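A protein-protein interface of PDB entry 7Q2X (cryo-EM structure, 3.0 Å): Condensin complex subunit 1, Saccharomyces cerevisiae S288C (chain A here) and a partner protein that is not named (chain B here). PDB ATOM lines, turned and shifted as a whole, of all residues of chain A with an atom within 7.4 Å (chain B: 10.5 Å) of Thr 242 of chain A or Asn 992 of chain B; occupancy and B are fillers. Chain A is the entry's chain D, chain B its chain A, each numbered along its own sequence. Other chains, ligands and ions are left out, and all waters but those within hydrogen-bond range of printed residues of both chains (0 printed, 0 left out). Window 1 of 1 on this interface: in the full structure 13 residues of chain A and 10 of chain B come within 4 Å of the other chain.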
ATOM      1  N   ARG A 198      10.840   6.896  23.991  1.00  0.00           N
ATOM      2  CA  ARG A 198      10.262   6.751  22.655  1.00  0.00           C
ATOM      3  C   ARG A 198       9.126   5.737  22.591  1.00  0.00           C
ATOM      4  O   ARG A 198       8.072   6.069  22.020  1.00  0.00           O
ATOM      5  CB  ARG A 198      11.370   6.403  21.656  1.00  0.00           C
ATOM      6  CG  ARG A 198      12.098   7.603  21.081  1.00  0.00           C
ATOM      7  CD  ARG A 198      13.534   7.241  20.726  1.00  0.00           C
ATOM      8  NE  ARG A 198      13.628   6.350  19.574  1.00  0.00           N
ATOM      9  CZ  ARG A 198      13.210   6.634  18.347  1.00  0.00           C
ATOM     10  NH1 ARG A 198      12.691   7.813  18.044  1.00  0.00           N
ATOM     11  NH2 ARG A 198      13.324   5.712  17.396  1.00  0.00           N
ATOM     12  N   VAL A 202       5.272   6.493  21.251  1.00  0.00           N
ATOM     13  CA  VAL A 202       4.614   5.797  20.149  1.00  0.00           C
ATOM     14  C   VAL A 202       3.303   5.165  20.602  1.00  0.00           C
ATOM     15  O   VAL A 202       2.310   5.184  19.865  1.00  0.00           O
ATOM     16  CB  VAL A 202       5.553   4.746  19.525  1.00  0.00           C
ATOM     17  CG1 VAL A 202       4.969   4.227  18.224  1.00  0.00           C
ATOM     18  CG2 VAL A 202       6.920   5.348  19.266  1.00  0.00           C
ATOM     19  N   GLU A 205      -0.004   7.236  20.775  1.00  0.00           N
ATOM     20  CA  GLU A 205      -0.666   7.665  19.546  1.00  0.00           C
ATOM     21  C   GLU A 205      -2.134   7.254  19.523  1.00  0.00           C
ATOM     22  O   GLU A 205      -2.998   8.037  19.109  1.00  0.00           O
ATOM     23  CB  GLU A 205       0.066   7.089  18.334  1.00  0.00           C
ATOM     24  CG  GLU A 205       1.450   7.673  18.099  1.00  0.00           C
ATOM     25  CD  GLU A 205       1.787   7.798  16.627  1.00  0.00           C
ATOM     26  OE1 GLU A 205       1.032   7.254  15.794  1.00  0.00           O
ATOM     27  OE2 GLU A 205       2.808   8.439  16.302  1.00  0.00           O
ATOM     28  N   SER A 235      14.410  17.257  23.842  1.00  0.00           N
ATOM     29  CA  SER A 235      13.808  16.129  23.137  1.00  0.00           C
ATOM     30  C   SER A 235      12.344  15.958  23.524  1.00  0.00           C
ATOM     31  O   SER A 235      11.487  15.712  22.666  1.00  0.00           O
ATOM     32  CB  SER A 235      14.596  14.852  23.424  1.00  0.00           C
ATOM     33  OG  SER A 235      14.424  14.438  24.768  1.00  0.00           O
ATOM     34  N   ILE A 236      12.038  16.084  24.817  1.00  0.00           N
ATOM     35  CA  ILE A 236      10.665  15.910  25.276  1.00  0.00           C
ATOM     36  C   ILE A 236       9.757  16.990  24.703  1.00  0.00           C
ATOM     37  O   ILE A 236       8.635  16.699  24.273  1.00  0.00           O
ATOM     38  CB  ILE A 236      10.611  15.886  26.814  1.00  0.00           C
ATOM     39  CG1 ILE A 236      11.557  14.815  27.361  1.00  0.00           C
ATOM     40  CG2 ILE A 236       9.191  15.632  27.293  1.00  0.00           C
ATOM     41  CD1 ILE A 236      11.214  13.412  26.910  1.00  0.00           C
ATOM     42  N   GLN A 237      10.212  18.246  24.692  1.00  0.00           N
ATOM     43  CA  GLN A 237       9.383  19.319  24.150  1.00  0.00           C
ATOM     44  C   GLN A 237       9.139  19.129  22.658  1.00  0.00           C
ATOM     45  O   GLN A 237       8.034  19.384  22.167  1.00  0.00           O
ATOM     46  CB  GLN A 237      10.024  20.680  24.440  1.00  0.00           C
ATOM     47  CG  GLN A 237      11.257  21.013  23.618  1.00  0.00           C
ATOM     48  CD  GLN A 237      11.465  22.504  23.461  1.00  0.00           C
ATOM     49  OE1 GLN A 237      10.681  23.308  23.966  1.00  0.00           O
ATOM     50  NE2 GLN A 237      12.525  22.885  22.757  1.00  0.00           N
ATOM     51  N   SER A 238      10.153  18.667  21.922  1.00  0.00           N
ATOM     52  CA  SER A 238       9.970  18.398  20.500  1.00  0.00           C
ATOM     53  C   SER A 238       8.991  17.252  20.277  1.00  0.00           C
ATOM     54  O   SER A 238       8.167  17.303  19.357  1.00  0.00           O
ATOM     55  CB  SER A 238      11.314  18.090  19.845  1.00  0.00           C
ATOM     56  OG  SER A 238      11.160  17.818  18.464  1.00  0.00           O
ATOM     57  N   SER A 239       9.072  16.206  21.103  1.00  0.00           N
ATOM     58  CA  SER A 239       8.123  15.104  20.987  1.00  0.00           C
ATOM     59  C   SER A 239       6.701  15.571  21.273  1.00  0.00           C
ATOM     60  O   SER A 239       5.759  15.184  20.570  1.00  0.00           O
ATOM     61  CB  SER A 239       8.518  13.970  21.933  1.00  0.00           C
ATOM     62  OG  SER A 239       9.799  13.460  21.610  1.00  0.00           O
ATOM     63  N   LEU A 240       6.525  16.402  22.303  1.00  0.00           N
ATOM     64  CA  LEU A 240       5.197  16.924  22.610  1.00  0.00           C
ATOM     65  C   LEU A 240       4.679  17.806  21.480  1.00  0.00           C
ATOM     66  O   LEU A 240       3.492  17.750  21.140  1.00  0.00           O
ATOM     67  CB  LEU A 240       5.216  17.697  23.929  1.00  0.00           C
ATOM     68  CG  LEU A 240       5.673  16.944  25.181  1.00  0.00           C
ATOM     69  CD1 LEU A 240       6.220  17.912  26.219  1.00  0.00           C
ATOM     70  CD2 LEU A 240       4.557  16.094  25.766  1.00  0.00           C
ATOM     71  N   MET A 241       5.552  18.623  20.887  1.00  0.00           N
ATOM     72  CA  MET A 241       5.143  19.444  19.751  1.00  0.00           C
ATOM     73  C   MET A 241       4.727  18.579  18.568  1.00  0.00           C
ATOM     74  O   MET A 241       3.726  18.867  17.902  1.00  0.00           O
ATOM     75  CB  MET A 241       6.273  20.391  19.352  1.00  0.00           C
ATOM     76  CG  MET A 241       5.827  21.558  18.486  1.00  0.00           C
ATOM     77  SD  MET A 241       4.667  22.648  19.331  1.00  0.00           S
ATOM     78  CE  MET A 241       5.692  23.271  20.660  1.00  0.00           C
ATOM     79  N   THR A 242       5.484  17.514  18.294  1.00  0.00           N
ATOM     80  CA  THR A 242       5.123  16.598  17.215  1.00  0.00           C
ATOM     81  C   THR A 242       3.765  15.954  17.469  1.00  0.00           C
ATOM     82  O   THR A 242       2.914  15.901  16.571  1.00  0.00           O
ATOM     83  CB  THR A 242       6.205  15.527  17.063  1.00  0.00           C
ATOM     84  OG1 THR A 242       7.450  16.145  16.712  1.00  0.00           O
ATOM     85  CG2 THR A 242       5.826  14.517  15.993  1.00  0.00           C
ATOM     86  N   ASN A 243       3.541  15.473  18.695  1.00  0.00           N
ATOM     87  CA  ASN A 243       2.267  14.843  19.024  1.00  0.00           C
ATOM     88  C   ASN A 243       1.116  15.833  18.914  1.00  0.00           C
ATOM     89  O   ASN A 243       0.027  15.483  18.448  1.00  0.00           O
ATOM     90  CB  ASN A 243       2.323  14.244  20.429  1.00  0.00           C
ATOM     91  CG  ASN A 243       3.453  13.250  20.593  1.00  0.00           C
ATOM     92  OD1 ASN A 243       3.922  12.659  19.622  1.00  0.00           O
ATOM     93  ND2 ASN A 243       3.900  13.065  21.828  1.00  0.00           N
ATOM     94  N   LEU A 244       1.338  17.076  19.342  1.00  0.00           N
ATOM     95  CA  LEU A 244       0.271  18.067  19.305  1.00  0.00           C
ATOM     96  C   LEU A 244      -0.016  18.528  17.881  1.00  0.00           C
ATOM     97  O   LEU A 244      -1.156  18.879  17.564  1.00  0.00           O
ATOM     98  CB  LEU A 244       0.635  19.245  20.210  1.00  0.00           C
ATOM     99  CG  LEU A 244      -0.365  20.384  20.385  1.00  0.00           C
ATOM    100  CD1 LEU A 244      -1.635  19.863  21.025  1.00  0.00           C
ATOM    101  CD2 LEU A 244       0.253  21.453  21.265  1.00  0.00           C
ATOM    102  N   THR A 245       0.995  18.528  17.010  1.00  0.00           N
ATOM    103  CA  THR A 245       0.765  18.890  15.616  1.00  0.00           C
ATOM    104  C   THR A 245       0.054  17.771  14.860  1.00  0.00           C
ATOM    105  O   THR A 245      -0.855  18.030  14.064  1.00  0.00           O
ATOM    106  CB  THR A 245       2.087  19.240  14.932  1.00  0.00           C
ATOM    107  OG1 THR A 245       3.038  18.191  15.157  1.00  0.00           O
ATOM    108  CG2 THR A 245       2.636  20.555  15.468  1.00  0.00           C
ATOM    109  N   TYR A 246       0.456  16.522  15.091  1.00  0.00           N
ATOM    110  CA  TYR A 246      -0.084  15.392  14.343  1.00  0.00           C
ATOM    111  C   TYR A 246      -1.376  14.830  14.924  1.00  0.00           C
ATOM    112  O   TYR A 246      -2.052  14.054  14.242  1.00  0.00           O
ATOM    113  CB  TYR A 246       0.959  14.274  14.247  1.00  0.00           C
ATOM    114  CG  TYR A 246       2.042  14.528  13.225  1.00  0.00           C
ATOM    115  CD1 TYR A 246       1.763  14.492  11.865  1.00  0.00           C
ATOM    116  CD2 TYR A 246       3.343  14.799  13.617  1.00  0.00           C
ATOM    117  CE1 TYR A 246       2.752  14.722  10.927  1.00  0.00           C
ATOM    118  CE2 TYR A 246       4.338  15.031  12.688  1.00  0.00           C
ATOM    119  CZ  TYR A 246       4.037  14.990  11.345  1.00  0.00           C
ATOM    120  OH  TYR A 246       5.027  15.222  10.418  1.00  0.00           O
ATOM    121  N   PHE A 247      -1.742  15.196  16.150  1.00  0.00           N
ATOM    122  CA  PHE A 247      -2.913  14.631  16.804  1.00  0.00           C
ATOM    123  C   PHE A 247      -3.699  15.721  17.519  1.00  0.00           C
ATOM    124  O   PHE A 247      -3.163  16.778  17.860  1.00  0.00           O
ATOM    125  CB  PHE A 247      -2.525  13.529  17.800  1.00  0.00           C
ATOM    126  CG  PHE A 247      -1.540  12.537  17.252  1.00  0.00           C
ATOM    127  CD1 PHE A 247      -1.918  11.645  16.263  1.00  0.00           C
ATOM    128  CD2 PHE A 247      -0.239  12.498  17.721  1.00  0.00           C
ATOM    129  CE1 PHE A 247      -1.017  10.733  15.753  1.00  0.00           C
ATOM    130  CE2 PHE A 247       0.668  11.588  17.215  1.00  0.00           C
ATOM    131  CZ  PHE A 247       0.278  10.706  16.230  1.00  0.00           C
ATOM    132  N   LEU A 250      -4.289  14.829  22.216  1.00  0.00           N
ATOM    133  CA  LEU A 250      -3.182  14.907  23.158  1.00  0.00           C
ATOM    134  C   LEU A 250      -2.960  16.314  23.705  1.00  0.00           C
ATOM    135  O   LEU A 250      -2.008  16.527  24.462  1.00  0.00           O
ATOM    136  CB  LEU A 250      -1.900  14.389  22.504  1.00  0.00           C
ATOM    137  CG  LEU A 250      -1.775  12.865  22.476  1.00  0.00           C
ATOM    138  CD1 LEU A 250      -0.423  12.437  21.934  1.00  0.00           C
ATOM    139  CD2 LEU A 250      -2.014  12.282  23.862  1.00  0.00           C
ATOM    140  N   ARG A 281       5.696  29.282  15.804  1.00  0.00           N
ATOM    141  CA  ARG A 281       5.288  28.210  14.905  1.00  0.00           C
ATOM    142  C   ARG A 281       4.545  28.770  13.695  1.00  0.00           C
ATOM    143  O   ARG A 281       3.804  29.752  13.789  1.00  0.00           O
ATOM    144  CB  ARG A 281       4.406  27.202  15.646  1.00  0.00           C
ATOM    145  CG  ARG A 281       3.830  26.100  14.771  1.00  0.00           C
ATOM    146  CD  ARG A 281       3.826  24.759  15.486  1.00  0.00           C
ATOM    147  NE  ARG A 281       3.730  23.647  14.548  1.00  0.00           N
ATOM    148  CZ  ARG A 281       4.774  23.026  14.014  1.00  0.00           C
ATOM    149  NH1 ARG A 281       6.013  23.369  14.323  1.00  0.00           N
ATOM    150  NH2 ARG A 281       4.568  22.035  13.152  1.00  0.00           N
ATOM    151  N   ILE B 203       8.977  17.855  -0.224  1.00  0.00           N
ATOM    152  CA  ILE B 203       9.677  16.957   0.686  1.00  0.00           C
ATOM    153  C   ILE B 203      11.026  16.534   0.116  1.00  0.00           C
ATOM    154  O   ILE B 203      12.029  16.513   0.839  1.00  0.00           O
ATOM    155  CB  ILE B 203       8.792  15.742   1.013  1.00  0.00           C
ATOM    156  CG1 ILE B 203       7.442  16.206   1.561  1.00  0.00           C
ATOM    157  CG2 ILE B 203       9.495  14.823   2.004  1.00  0.00           C
ATOM    158  CD1 ILE B 203       6.647  15.116   2.234  1.00  0.00           C
ATOM    159  N   LEU B 207      13.975  16.381   2.170  1.00  0.00           N
ATOM    160  CA  LEU B 207      14.476  15.071   2.573  1.00  0.00           C
ATOM    161  C   LEU B 207      15.962  14.931   2.271  1.00  0.00           C
ATOM    162  O   LEU B 207      16.726  14.432   3.106  1.00  0.00           O
ATOM    163  CB  LEU B 207      13.681  13.967   1.876  1.00  0.00           C
ATOM    164  CG  LEU B 207      13.759  12.576   2.508  1.00  0.00           C
ATOM    165  CD1 LEU B 207      13.383  12.634   3.981  1.00  0.00           C
ATOM    166  CD2 LEU B 207      12.870  11.595   1.760  1.00  0.00           C
ATOM    167  N   LEU B 210      17.958  17.033   4.737  1.00  0.00           N
ATOM    168  CA  LEU B 210      18.069  16.363   6.031  1.00  0.00           C
ATOM    169  C   LEU B 210      19.055  15.202   5.969  1.00  0.00           C
ATOM    170  O   LEU B 210      19.834  14.988   6.905  1.00  0.00           O
ATOM    171  CB  LEU B 210      16.693  15.885   6.492  1.00  0.00           C
ATOM    172  CG  LEU B 210      15.686  16.995   6.807  1.00  0.00           C
ATOM    173  CD1 LEU B 210      14.314  16.419   7.119  1.00  0.00           C
ATOM    174  CD2 LEU B 210      16.183  17.859   7.956  1.00  0.00           C
ATOM    175  N   ASN B 985      18.354  16.480  18.673  1.00  0.00           N
ATOM    176  CA  ASN B 985      17.281  15.493  18.681  1.00  0.00           C
ATOM    177  C   ASN B 985      16.659  15.299  17.301  1.00  0.00           C
ATOM    178  O   ASN B 985      15.449  15.081  17.188  1.00  0.00           O
ATOM    179  CB  ASN B 985      16.220  15.887  19.706  1.00  0.00           C
ATOM    180  CG  ASN B 985      15.566  17.216  19.388  1.00  0.00           C
ATOM    181  OD1 ASN B 985      16.064  17.987  18.569  1.00  0.00           O
ATOM    182  ND2 ASN B 985      14.452  17.497  20.050  1.00  0.00           N
ATOM    183  N   ILE B 986      17.473  15.376  16.243  1.00  0.00           N
ATOM    184  CA  ILE B 986      16.965  15.236  14.883  1.00  0.00           C
ATOM    185  C   ILE B 986      16.502  13.815  14.580  1.00  0.00           C
ATOM    186  O   ILE B 986      15.693  13.616  13.667  1.00  0.00           O
ATOM    187  CB  ILE B 986      18.040  15.681  13.871  1.00  0.00           C
ATOM    188  CG1 ILE B 986      17.409  16.033  12.522  1.00  0.00           C
ATOM    189  CG2 ILE B 986      19.105  14.607  13.701  1.00  0.00           C
ATOM    190  CD1 ILE B 986      16.737  17.382  12.501  1.00  0.00           C
ATOM    191  N   MET B 987      16.991  12.821  15.328  1.00  0.00           N
ATOM    192  CA  MET B 987      16.700  11.428  14.996  1.00  0.00           C
ATOM    193  C   MET B 987      15.211  11.123  15.106  1.00  0.00           C
ATOM    194  O   MET B 987      14.644  10.442  14.242  1.00  0.00           O
ATOM    195  CB  MET B 987      17.506  10.498  15.904  1.00  0.00           C
ATOM    196  CG  MET B 987      19.007  10.548  15.671  1.00  0.00           C
ATOM    197  SD  MET B 987      19.459  10.236  13.955  1.00  0.00           S
ATOM    198  CE  MET B 987      20.956   9.277  14.170  1.00  0.00           C
ATOM    199  N   ASN B 988      14.563  11.614  16.165  1.00  0.00           N
ATOM    200  CA  ASN B 988      13.143  11.336  16.356  1.00  0.00           C
ATOM    201  C   ASN B 988      12.306  11.928  15.229  1.00  0.00           C
ATOM    202  O   ASN B 988      11.411  11.264  14.693  1.00  0.00           O
ATOM    203  CB  ASN B 988      12.682  11.877  17.709  1.00  0.00           C
ATOM    204  CG  ASN B 988      13.394  11.217  18.873  1.00  0.00           C
ATOM    205  OD1 ASN B 988      14.226  10.330  18.685  1.00  0.00           O
ATOM    206  ND2 ASN B 988      13.070  11.648  20.086  1.00  0.00           N
ATOM    207  N   MET B 989      12.589  13.177  14.848  1.00  0.00           N
ATOM    208  CA  MET B 989      11.815  13.807  13.785  1.00  0.00           C
ATOM    209  C   MET B 989      12.092  13.147  12.441  1.00  0.00           C
ATOM    210  O   MET B 989      11.183  13.005  11.616  1.00  0.00           O
ATOM    211  CB  MET B 989      12.109  15.306  13.725  1.00  0.00           C
ATOM    212  CG  MET B 989      11.291  16.044  12.674  1.00  0.00           C
ATOM    213  SD  MET B 989      11.606  17.818  12.611  1.00  0.00           S
ATOM    214  CE  MET B 989      13.239  17.849  11.884  1.00  0.00           C
ATOM    215  N   ILE B 990      13.338  12.726  12.203  1.00  0.00           N
ATOM    216  CA  ILE B 990      13.657  12.014  10.968  1.00  0.00           C
ATOM    217  C   ILE B 990      12.879  10.706  10.891  1.00  0.00           C
ATOM    218  O   ILE B 990      12.306  10.367   9.847  1.00  0.00           O
ATOM    219  CB  ILE B 990      15.176  11.777  10.862  1.00  0.00           C
ATOM    220  CG1 ILE B 990      15.903  13.088  10.561  1.00  0.00           C
ATOM    221  CG2 ILE B 990      15.486  10.741   9.794  1.00  0.00           C
ATOM    222  CD1 ILE B 990      15.474  13.735   9.268  1.00  0.00           C
ATOM    223  N   GLU B 991      12.843   9.954  11.994  1.00  0.00           N
ATOM    224  CA  GLU B 991      12.104   8.695  12.005  1.00  0.00           C
ATOM    225  C   GLU B 991      10.611   8.929  11.803  1.00  0.00           C
ATOM    226  O   GLU B 991       9.952   8.185  11.065  1.00  0.00           O
ATOM    227  CB  GLU B 991      12.360   7.948  13.313  1.00  0.00           C
ATOM    228  CG  GLU B 991      13.753   7.350  13.421  1.00  0.00           C
ATOM    229  CD  GLU B 991      13.761   6.011  14.132  1.00  0.00           C
ATOM    230  OE1 GLU B 991      12.669   5.516  14.483  1.00  0.00           O
ATOM    231  OE2 GLU B 991      14.858   5.452  14.337  1.00  0.00           O
ATOM    232  N   ASN B 992      10.060   9.960  12.450  1.00  0.00           N
ATOM    233  CA  ASN B 992       8.643  10.265  12.278  1.00  0.00           C
ATOM    234  C   ASN B 992       8.332  10.652  10.837  1.00  0.00           C
ATOM    235  O   ASN B 992       7.311  10.232  10.280  1.00  0.00           O
ATOM    236  CB  ASN B 992       8.225  11.380  13.237  1.00  0.00           C
ATOM    237  CG  ASN B 992       8.277  10.948  14.689  1.00  0.00           C
ATOM    238  OD1 ASN B 992       7.901   9.826  15.029  1.00  0.00           O
ATOM    239  ND2 ASN B 992       8.745  11.839  15.554  1.00  0.00           N
ATOM    240  N   VAL B 993       9.203  11.452  10.217  1.00  0.00           N
ATOM    241  CA  VAL B 993       8.992  11.861   8.832  1.00  0.00           C
ATOM    242  C   VAL B 993       9.059  10.656   7.904  1.00  0.00           C
ATOM    243  O   VAL B 993       8.261  10.529   6.968  1.00  0.00           O
ATOM    244  CB  VAL B 993      10.013  12.946   8.438  1.00  0.00           C
ATOM    245  CG1 VAL B 993      10.133  13.053   6.924  1.00  0.00           C
ATOM    246  CG2 VAL B 993       9.618  14.282   9.043  1.00  0.00           C
ATOM    247  N   GLU B 994      10.011   9.751   8.147  1.00  0.00           N
ATOM    248  CA  GLU B 994      10.103   8.541   7.334  1.00  0.00           C
ATOM    249  C   GLU B 994       8.850   7.684   7.476  1.00  0.00           C
ATOM    250  O   GLU B 994       8.331   7.157   6.482  1.00  0.00           O
ATOM    251  CB  GLU B 994      11.346   7.742   7.725  1.00  0.00           C
ATOM    252  CG  GLU B 994      11.724   6.655   6.733  1.00  0.00           C
ATOM    253  CD  GLU B 994      13.091   6.061   7.014  1.00  0.00           C
ATOM    254  OE1 GLU B 994      13.738   6.493   7.992  1.00  0.00           O
ATOM    255  OE2 GLU B 994      13.517   5.162   6.260  1.00  0.00           O
ATOM    256  N   LYS B 995       8.349   7.534   8.706  1.00  0.00           N
ATOM    257  CA  LYS B 995       7.132   6.757   8.919  1.00  0.00           C
ATOM    258  C   LYS B 995       5.941   7.389   8.208  1.00  0.00           C
ATOM    259  O   LYS B 995       5.138   6.689   7.579  1.00  0.00           O
ATOM    260  CB  LYS B 995       6.855   6.618  10.416  1.00  0.00           C
ATOM    261  CG  LYS B 995       5.654   5.749  10.750  1.00  0.00           C
ATOM    262  CD  LYS B 995       5.473   5.614  12.252  1.00  0.00           C
ATOM    263  CE  LYS B 995       4.328   4.672  12.590  1.00  0.00           C
ATOM    264  NZ  LYS B 995       3.010   5.232  12.186  1.00  0.00           N
ATOM    265  N   LYS B 996       5.814   8.716   8.293  1.00  0.00           N
ATOM    266  CA  LYS B 996       4.713   9.398   7.618  1.00  0.00           C
ATOM    267  C   LYS B 996       4.818   9.258   6.105  1.00  0.00           C
ATOM    268  O   LYS B 996       3.804   9.076   5.421  1.00  0.00           O
ATOM    269  CB  LYS B 996       4.678  10.872   8.021  1.00  0.00           C
ATOM    270  CG  LYS B 996       4.378  11.110   9.492  1.00  0.00           C
ATOM    271  CD  LYS B 996       2.886  11.067   9.771  1.00  0.00           C
ATOM    272  CE  LYS B 996       2.607  11.019  11.264  1.00  0.00           C
ATOM    273  NZ  LYS B 996       3.139   9.777  11.891  1.00  0.00           N
ATOM    274  N   GLU B 997       6.035   9.346   5.562  1.00  0.00           N
ATOM    275  CA  GLU B 997       6.220   9.182   4.124  1.00  0.00           C
ATOM    276  C   GLU B 997       5.848   7.774   3.677  1.00  0.00           C
ATOM    277  O   GLU B 997       5.196   7.595   2.640  1.00  0.00           O
ATOM    278  CB  GLU B 997       7.663   9.505   3.742  1.00  0.00           C
ATOM    279  CG  GLU B 997       7.942   9.441   2.250  1.00  0.00           C
ATOM    280  CD  GLU B 997       9.370   9.816   1.911  1.00  0.00           C
ATOM    281  OE1 GLU B 997      10.147  10.105   2.845  1.00  0.00           O
ATOM    282  OE2 GLU B 997       9.717   9.821   0.711  1.00  0.00           O
ATOM    283  N   ALA B 998       6.255   6.760   4.445  1.00  0.00           N
ATOM    284  CA  ALA B 998       5.881   5.389   4.111  1.00  0.00           C
ATOM    285  C   ALA B 998       4.371   5.200   4.172  1.00  0.00           C
ATOM    286  O   ALA B 998       3.782   4.537   3.306  1.00  0.00           O
ATOM    287  CB  ALA B 998       6.585   4.409   5.050  1.00  0.00           C
ATOM    288  N   ALA B 999       3.726   5.780   5.188  1.00  0.00           N
ATOM    289  CA  ALA B 999       2.274   5.684   5.291  1.00  0.00           C
ATOM    290  C   ALA B 999       1.593   6.347   4.101  1.00  0.00           C
ATOM    291  O   ALA B 999       0.634   5.801   3.544  1.00  0.00           O
ATOM    292  CB  ALA B 999       1.797   6.308   6.602  1.00  0.00           C
ATOM    293  N   LEU B1000       2.079   7.523   3.694  1.00  0.00           N
ATOM    294  CA  LEU B1000       1.503   8.203   2.538  1.00  0.00           C
ATOM    295  C   LEU B1000       1.690   7.389   1.264  1.00  0.00           C
ATOM    296  O   LEU B1000       0.786   7.325   0.423  1.00  0.00           O
ATOM    297  CB  LEU B1000       2.122   9.592   2.380  1.00  0.00           C
ATOM    298  CG  LEU B1000       1.537  10.685   3.273  1.00  0.00           C
ATOM    299  CD1 LEU B1000       2.500  11.851   3.390  1.00  0.00           C
ATOM    300  CD2 LEU B1000       0.200  11.147   2.722  1.00  0.00           C
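OD1 of Asn 988 of chain B sits at hydrogen-bond distance from NH1 of Arg 198 of chain A, at 3.0 Å.
NH2 of Arg 198 of chain A lies within salt-bridge range of OE1 of Glu 991 of chain B (3.0 Å).
ND2 of Asn 992 of chain B lies within hydrogen-bond range of O of Asn 988 of chain B.
The backbone carbonyl oxygen of Ser 235 of chain A is in hydrogen-bond range of the side-chain hydroxyl of Ser 239 of chain A, 3.0 Å away.
The backbone carbonyl oxygen of Ser 238 of chain A is in hydrogen-bond range of the side-chain hydroxyl of Thr 242 of chain A (3.0 Å).
The backbone carbonyl oxygen (O) of Thr 242 of chain A sits at hydrogen-bond distance from the side-chain hydroxyl (OG1) of Thr 245 of chain A, 2.7 Å away.
Ser 235 of chain A touches Asn 985 of chain B (CA to ND2, 3.4 Å).
Asn 985 of chain B touches Ser 238 of chain A.
CG2 of Thr 242 of chain A touches ND2 of Asn 992 of chain B, 3.99 Å away.
Lys 996 of chain B touches Tyr 246 of chain A.
Of the printed residues of chain B, Arg 198 of chain A touches Asn 988 and Glu 991.
Of the printed residues of chain B, Ser 235 of chain A touches Asn 985.
Of chain B, only Asn 985 (3.2 Å) comes within 4 Å of Ser 238 of chain A.
Printed residues of chain B within 4 Å of Thr 242 of chain A: Asn 992 (3.99 Å).
No residue of chain B comes within 4 Å of Thr 245 of chain A.
Tyr 246 of chain A touches one residue of chain B.
Leu 210 of chain B touches none of the printed residues of chain A.
Of the printed residues of chain A, Asn 985 of chain B touches Ser 235 and Ser 238.
Met 989 of chain B touches none of the printed residues of chain A.
Printed residues of chain A within 4 Å of Asn 992 of chain B: Thr 242 (3.99 Å).
Printed residues of chain A within 4 Å of Lys 996 of chain B: Tyr 246 (3.6 Å).
The nearest printed residue of chain B that does not touch Thr 242 of chain A is Met 989 of chain B (5.6 Å).
The nearest printed residue of chain A that does not touch Asn 992 of chain B is Tyr 246 of chain A (5.4 Å).
The nearest printed residue of chain A that does not touch Lys 996 of chain B is Glu 205 of chain A (4.6 Å).
Of the 19 printed residues of chain B, 5 touch a printed residue of chain A.
Of the 18 printed residues of chain A, 5 touch a printed residue of chain B.
Among the printed residues, 6 pairs touch across the chains.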
